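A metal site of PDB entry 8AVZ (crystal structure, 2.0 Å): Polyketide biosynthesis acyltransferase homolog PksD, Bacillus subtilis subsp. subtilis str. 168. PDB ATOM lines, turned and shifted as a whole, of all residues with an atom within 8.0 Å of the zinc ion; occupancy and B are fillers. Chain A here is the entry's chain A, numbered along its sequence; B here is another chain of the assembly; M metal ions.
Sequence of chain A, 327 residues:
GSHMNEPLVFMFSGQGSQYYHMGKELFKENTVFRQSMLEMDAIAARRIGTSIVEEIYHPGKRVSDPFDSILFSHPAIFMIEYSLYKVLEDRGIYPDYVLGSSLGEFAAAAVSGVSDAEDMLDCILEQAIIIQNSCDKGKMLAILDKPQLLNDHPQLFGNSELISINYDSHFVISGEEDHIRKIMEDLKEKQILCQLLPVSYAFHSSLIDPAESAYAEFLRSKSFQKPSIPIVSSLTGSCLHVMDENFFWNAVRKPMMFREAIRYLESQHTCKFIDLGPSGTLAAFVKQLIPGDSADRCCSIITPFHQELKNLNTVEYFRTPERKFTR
SG of Cys 239 of chain B sits close to OH of Tyr 264 of chain A.
The side-chain hydroxyl (OG) of Ser 238 of chain B lies close to the side-chain sulfur (SG) of Cys 239 of chain B, 3.5 Å away.
The backbone carbonyl oxygen of Cys 239 of chain A sits at hydrogen-bond distance from the side-chain hydroxyl of Tyr 264 of chain B (3.0 Å).
The side-chain sulfur of Cys 239 of chain B lies close to the side-chain hydroxyl of Tyr 264 of chain B (3.8 Å).
The backbone NH (N) of His 241 of chain A lies within hydrogen-bond range of the side-chain amide oxygen (OE1) of Gln 268 of chain B (2.7 Å).
A ring nitrogen (ND1) of His 241 of chain A lies within hydrogen-bond range of the side-chain hydroxyl of Tyr 97 of chain B, at 3.0 Å.
O of Ile 231 of chain A lies close to SG of Cys 239 of chain A (3.7 Å).
A ring nitrogen (NE2) of His 241 of chain A lies close to the side-chain hydroxyl (OH) of Tyr 264 of chain B, 3.1 Å away.
Tyr 264 of chain B touches the zinc ion.
The zinc ion is bound by a ring nitrogen (NE2) of His 241 of chain A, a ring nitrogen (NE2) of His 241 of chain B, the side-chain sulfur of Cys 239 of chain B and the side-chain sulfur of Cys 239 of chain A.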
ATOM      1  N   TYR A  97      16.585  27.624  12.752  1.00  0.00           N
ATOM      2  CA  TYR A  97      16.814  26.819  11.566  1.00  0.00           C
ATOM      3  C   TYR A  97      18.106  26.068  11.793  1.00  0.00           C
ATOM      4  O   TYR A  97      19.000  26.572  12.449  1.00  0.00           O
ATOM      5  CB  TYR A  97      17.011  27.684  10.302  1.00  0.00           C
ATOM      6  CG  TYR A  97      15.846  28.565   9.917  1.00  0.00           C
ATOM      7  CD1 TYR A  97      15.722  29.865  10.428  1.00  0.00           C
ATOM      8  CD2 TYR A  97      14.923  28.126   8.975  1.00  0.00           C
ATOM      9  CE1 TYR A  97      14.677  30.678  10.052  1.00  0.00           C
ATOM     10  CE2 TYR A  97      13.845  28.943   8.617  1.00  0.00           C
ATOM     11  CZ  TYR A  97      13.745  30.215   9.152  1.00  0.00           C
ATOM     12  OH  TYR A  97      12.706  31.035   8.780  1.00  0.00           O
ATOM     13  N   PRO A 227      11.007  16.584   9.886  1.00  0.00           N
ATOM     14  CA  PRO A 227      11.752  17.566  10.682  1.00  0.00           C
ATOM     15  C   PRO A 227      10.858  18.299  11.652  1.00  0.00           C
ATOM     16  O   PRO A 227       9.740  18.684  11.322  1.00  0.00           O
ATOM     17  CB  PRO A 227      12.320  18.534   9.628  1.00  0.00           C
ATOM     18  CG  PRO A 227      11.529  18.299   8.432  1.00  0.00           C
ATOM     19  CD  PRO A 227      11.059  16.883   8.440  1.00  0.00           C
ATOM     20  N   ILE A 229      12.576  20.902  13.556  1.00  0.00           N
ATOM     21  CA  ILE A 229      13.219  22.199  13.429  1.00  0.00           C
ATOM     22  C   ILE A 229      13.458  22.402  11.940  1.00  0.00           C
ATOM     23  O   ILE A 229      13.894  21.457  11.269  1.00  0.00           O
ATOM     24  CB  ILE A 229      14.539  22.249  14.231  1.00  0.00           C
ATOM     25  CG1 ILE A 229      14.234  22.060  15.727  1.00  0.00           C
ATOM     26  CG2 ILE A 229      15.265  23.596  14.020  1.00  0.00           C
ATOM     27  CD1 ILE A 229      15.474  21.846  16.588  1.00  0.00           C
ATOM     28  N   PRO A 230      13.097  23.551  11.374  1.00  0.00           N
ATOM     29  CA  PRO A 230      13.279  23.753   9.919  1.00  0.00           C
ATOM     30  C   PRO A 230      14.710  23.459   9.515  1.00  0.00           C
ATOM     31  O   PRO A 230      15.642  24.019  10.094  1.00  0.00           O
ATOM     32  CB  PRO A 230      12.952  25.236   9.716  1.00  0.00           C
ATOM     33  CG  PRO A 230      12.158  25.663  10.890  1.00  0.00           C
ATOM     34  CD  PRO A 230      12.543  24.755  12.047  1.00  0.00           C
ATOM     35  N   ILE A 231      14.897  22.535   8.567  1.00  0.00           N
ATOM     36  CA  ILE A 231      16.183  22.269   7.948  1.00  0.00           C
ATOM     37  C   ILE A 231      16.279  22.974   6.603  1.00  0.00           C
ATOM     38  O   ILE A 231      15.479  22.703   5.704  1.00  0.00           O
ATOM     39  CB  ILE A 231      16.386  20.773   7.715  1.00  0.00           C
ATOM     40  CG1 ILE A 231      16.013  19.976   8.960  1.00  0.00           C
ATOM     41  CG2 ILE A 231      17.769  20.535   7.121  1.00  0.00           C
ATOM     42  CD1 ILE A 231      16.083  18.457   8.744  1.00  0.00           C
ATOM     43  N   VAL A 232      17.310  23.817   6.447  1.00  0.00           N
ATOM     44  CA  VAL A 232      17.695  24.355   5.155  1.00  0.00           C
ATOM     45  C   VAL A 232      18.880  23.512   4.676  1.00  0.00           C
ATOM     46  O   VAL A 232      19.869  23.369   5.387  1.00  0.00           O
ATOM     47  CB  VAL A 232      18.062  25.839   5.238  1.00  0.00           C
ATOM     48  CG1 VAL A 232      18.625  26.356   3.887  1.00  0.00           C
ATOM     49  CG2 VAL A 232      16.862  26.689   5.646  1.00  0.00           C
ATOM     50  N   SER A 238      17.426  25.011  -0.152  1.00  0.00           N
ATOM     51  CA  SER A 238      16.210  25.582   0.393  1.00  0.00           C
ATOM     52  C   SER A 238      15.778  24.839   1.647  1.00  0.00           C
ATOM     53  O   SER A 238      16.381  23.845   2.060  1.00  0.00           O
ATOM     54  CB  SER A 238      15.068  25.580  -0.616  1.00  0.00           C
ATOM     55  OG  SER A 238      14.066  26.483  -0.181  1.00  0.00           O
ATOM     56  N   CYS A 239      14.688  25.353   2.242  1.00  0.00           N
ATOM     57  CA  CYS A 239      14.057  24.662   3.344  1.00  0.00           C
ATOM     58  C   CYS A 239      13.530  23.325   2.842  1.00  0.00           C
ATOM     59  O   CYS A 239      12.885  23.264   1.794  1.00  0.00           O
ATOM     60  CB  CYS A 239      12.921  25.507   3.940  1.00  0.00           C
ATOM     61  SG  CYS A 239      12.581  24.971   5.659  1.00  0.00           S
ATOM     62  N   LEU A 240      13.820  22.267   3.591  1.00  0.00           N
ATOM     63  CA  LEU A 240      13.518  20.905   3.156  1.00  0.00           C
ATOM     64  C   LEU A 240      12.509  20.315   4.134  1.00  0.00           C
ATOM     65  O   LEU A 240      12.853  20.051   5.292  1.00  0.00           O
ATOM     66  CB  LEU A 240      14.786  20.053   3.129  1.00  0.00           C
ATOM     67  CG  LEU A 240      14.723  18.827   2.220  1.00  0.00           C
ATOM     68  CD1 LEU A 240      14.151  19.167   0.836  1.00  0.00           C
ATOM     69  CD2 LEU A 240      16.079  18.183   2.134  1.00  0.00           C
ATOM     70  N   HIS A 241      11.271  20.102   3.667  1.00  0.00           N
ATOM     71  CA  HIS A 241      10.217  19.538   4.508  1.00  0.00           C
ATOM     72  C   HIS A 241      10.090  18.035   4.345  1.00  0.00           C
ATOM     73  O   HIS A 241       9.624  17.367   5.268  1.00  0.00           O
ATOM     74  CB  HIS A 241       8.863  20.201   4.226  1.00  0.00           C
ATOM     75  CG  HIS A 241       8.794  21.631   4.649  1.00  0.00           C
ATOM     76  ND1 HIS A 241       7.619  22.284   4.920  1.00  0.00           N
ATOM     77  CD2 HIS A 241       9.782  22.533   4.864  1.00  0.00           C
ATOM     78  CE1 HIS A 241       7.875  23.533   5.289  1.00  0.00           C
ATOM     79  NE2 HIS A 241       9.183  23.704   5.247  1.00  0.00           N
ATOM     80  N   TYR A 264      18.769  32.084   0.378  1.00  0.00           N
ATOM     81  CA  TYR A 264      17.395  31.803   0.779  1.00  0.00           C
ATOM     82  C   TYR A 264      17.104  32.325   2.186  1.00  0.00           C
ATOM     83  O   TYR A 264      16.079  32.995   2.426  1.00  0.00           O
ATOM     84  CB  TYR A 264      17.090  30.307   0.714  1.00  0.00           C
ATOM     85  CG  TYR A 264      15.731  30.025   1.259  1.00  0.00           C
ATOM     86  CD1 TYR A 264      14.615  30.282   0.472  1.00  0.00           C
ATOM     87  CD2 TYR A 264      15.546  29.534   2.562  1.00  0.00           C
ATOM     88  CE1 TYR A 264      13.335  30.056   0.950  1.00  0.00           C
ATOM     89  CE2 TYR A 264      14.255  29.304   3.058  1.00  0.00           C
ATOM     90  CZ  TYR A 264      13.159  29.564   2.242  1.00  0.00           C
ATOM     91  OH  TYR A 264      11.879  29.335   2.682  1.00  0.00           O
ATOM     92  N   TYR B  97      -0.880  21.765   6.198  1.00  0.00           N
ATOM     93  CA  TYR B  97      -0.371  23.106   5.987  1.00  0.00           C
ATOM     94  C   TYR B  97      -1.561  24.043   5.951  1.00  0.00           C
ATOM     95  O   TYR B  97      -2.643  23.649   5.525  1.00  0.00           O
ATOM     96  CB  TYR B  97       0.350  23.277   4.649  1.00  0.00           C
ATOM     97  CG  TYR B  97       1.666  22.560   4.498  1.00  0.00           C
ATOM     98  CD1 TYR B  97       2.844  23.189   4.861  1.00  0.00           C
ATOM     99  CD2 TYR B  97       1.726  21.293   3.947  1.00  0.00           C
ATOM    100  CE1 TYR B  97       4.091  22.536   4.700  1.00  0.00           C
ATOM    101  CE2 TYR B  97       2.941  20.640   3.767  1.00  0.00           C
ATOM    102  CZ  TYR B  97       4.106  21.260   4.158  1.00  0.00           C
ATOM    103  OH  TYR B  97       5.299  20.626   3.984  1.00  0.00           O
ATOM    104  N   PRO B 230       2.286  24.061  10.127  1.00  0.00           N
ATOM    105  CA  PRO B 230       3.178  24.676   9.128  1.00  0.00           C
ATOM    106  C   PRO B 230       2.412  25.644   8.226  1.00  0.00           C
ATOM    107  O   PRO B 230       1.310  25.340   7.755  1.00  0.00           O
ATOM    108  CB  PRO B 230       3.725  23.470   8.345  1.00  0.00           C
ATOM    109  CG  PRO B 230       3.631  22.322   9.353  1.00  0.00           C
ATOM    110  CD  PRO B 230       2.394  22.592  10.127  1.00  0.00           C
ATOM    111  N   ILE B 231       2.997  26.821   8.014  1.00  0.00           N
ATOM    112  CA  ILE B 231       2.397  27.885   7.228  1.00  0.00           C
ATOM    113  C   ILE B 231       3.175  27.999   5.927  1.00  0.00           C
ATOM    114  O   ILE B 231       4.416  27.996   5.920  1.00  0.00           O
ATOM    115  CB  ILE B 231       2.444  29.232   7.969  1.00  0.00           C
ATOM    116  CG1 ILE B 231       1.622  29.169   9.245  1.00  0.00           C
ATOM    117  CG2 ILE B 231       1.921  30.371   7.055  1.00  0.00           C
ATOM    118  CD1 ILE B 231       1.664  30.457  10.044  1.00  0.00           C
ATOM    119  N   VAL B 232       2.457  28.110   4.826  1.00  0.00           N
ATOM    120  CA  VAL B 232       3.028  28.588   3.571  1.00  0.00           C
ATOM    121  C   VAL B 232       2.341  29.919   3.285  1.00  0.00           C
ATOM    122  O   VAL B 232       1.130  30.040   3.476  1.00  0.00           O
ATOM    123  CB  VAL B 232       2.854  27.562   2.440  1.00  0.00           C
ATOM    124  CG1 VAL B 232       3.385  28.145   1.110  1.00  0.00           C
ATOM    125  CG2 VAL B 232       3.596  26.309   2.785  1.00  0.00           C
ATOM    126  N   SER B 238       6.893  31.166   0.184  1.00  0.00           N
ATOM    127  CA  SER B 238       7.544  29.949   0.662  1.00  0.00           C
ATOM    128  C   SER B 238       7.011  29.614   2.059  1.00  0.00           C
ATOM    129  O   SER B 238       6.149  30.308   2.609  1.00  0.00           O
ATOM    130  CB  SER B 238       9.088  30.070   0.663  1.00  0.00           C
ATOM    131  OG  SER B 238       9.762  28.881   1.139  1.00  0.00           O
ATOM    132  N   CYS B 239       7.525  28.524   2.621  1.00  0.00           N
ATOM    133  CA  CYS B 239       7.202  28.168   3.977  1.00  0.00           C
ATOM    134  C   CYS B 239       7.544  29.329   4.892  1.00  0.00           C
ATOM    135  O   CYS B 239       8.383  30.171   4.577  1.00  0.00           O
ATOM    136  CB  CYS B 239       7.916  26.854   4.351  1.00  0.00           C
ATOM    137  SG  CYS B 239       9.718  27.036   4.109  1.00  0.00           S
ATOM    138  N   LEU B 240       6.805  29.434   5.978  1.00  0.00           N
ATOM    139  CA  LEU B 240       6.997  30.546   6.879  1.00  0.00           C
ATOM    140  C   LEU B 240       7.182  29.958   8.271  1.00  0.00           C
ATOM    141  O   LEU B 240       6.236  29.406   8.857  1.00  0.00           O
ATOM    142  CB  LEU B 240       5.816  31.509   6.802  1.00  0.00           C
ATOM    143  CG  LEU B 240       6.159  32.759   7.605  1.00  0.00           C
ATOM    144  CD1 LEU B 240       5.771  33.991   6.893  1.00  0.00           C
ATOM    145  CD2 LEU B 240       5.480  32.660   8.924  1.00  0.00           C
ATOM    146  N   HIS B 241       8.402  30.006   8.777  1.00  0.00           N
ATOM    147  CA  HIS B 241       8.651  29.469  10.106  1.00  0.00           C
ATOM    148  C   HIS B 241       8.850  30.522  11.151  1.00  0.00           C
ATOM    149  O   HIS B 241       8.513  30.289  12.294  1.00  0.00           O
ATOM    150  CB  HIS B 241       9.870  28.533  10.100  1.00  0.00           C
ATOM    151  CG  HIS B 241       9.736  27.435   9.088  1.00  0.00           C
ATOM    152  ND1 HIS B 241       8.951  26.342   9.333  1.00  0.00           N
ATOM    153  CD2 HIS B 241      10.232  27.284   7.841  1.00  0.00           C
ATOM    154  CE1 HIS B 241       8.986  25.525   8.289  1.00  0.00           C
ATOM    155  NE2 HIS B 241       9.759  26.080   7.372  1.00  0.00           N
ATOM    156  N   TYR B 264       6.520  25.896  -4.396  1.00  0.00           N
ATOM    157  CA  TYR B 264       7.252  25.336  -3.255  1.00  0.00           C
ATOM    158  C   TYR B 264       6.579  24.083  -2.715  1.00  0.00           C
ATOM    159  O   TYR B 264       7.241  23.069  -2.456  1.00  0.00           O
ATOM    160  CB  TYR B 264       7.442  26.367  -2.130  1.00  0.00           C
ATOM    161  CG  TYR B 264       8.129  25.689  -0.950  1.00  0.00           C
ATOM    162  CD1 TYR B 264       9.529  25.515  -0.932  1.00  0.00           C
ATOM    163  CD2 TYR B 264       7.400  25.234   0.155  1.00  0.00           C
ATOM    164  CE1 TYR B 264      10.164  24.842   0.145  1.00  0.00           C
ATOM    165  CE2 TYR B 264       8.021  24.579   1.229  1.00  0.00           C
ATOM    166  CZ  TYR B 264       9.392  24.397   1.212  1.00  0.00           C
ATOM    167  OH  TYR B 264       9.988  23.765   2.270  1.00  0.00           O
ATOM    168  N   GLN B 268       7.858  19.741  -2.845  1.00  0.00           N
ATOM    169  CA  GLN B 268       8.057  18.868  -1.695  1.00  0.00           C
ATOM    170  C   GLN B 268       7.097  17.688  -1.669  1.00  0.00           C
ATOM    171  O   GLN B 268       7.458  16.606  -1.204  1.00  0.00           O
ATOM    172  CB  GLN B 268       7.880  19.623  -0.373  1.00  0.00           C
ATOM    173  CG  GLN B 268       8.694  20.863  -0.203  1.00  0.00           C
ATOM    174  CD  GLN B 268      10.148  20.557   0.007  1.00  0.00           C
ATOM    175  OE1 GLN B 268      10.560  20.075   1.059  1.00  0.00           O
ATOM    176  NE2 GLN B 268      10.951  20.910  -0.966  1.00  0.00           N
HETATM  177 ZN    ZN M   1      10.230  25.332   5.581  1.00  0.00          ZN
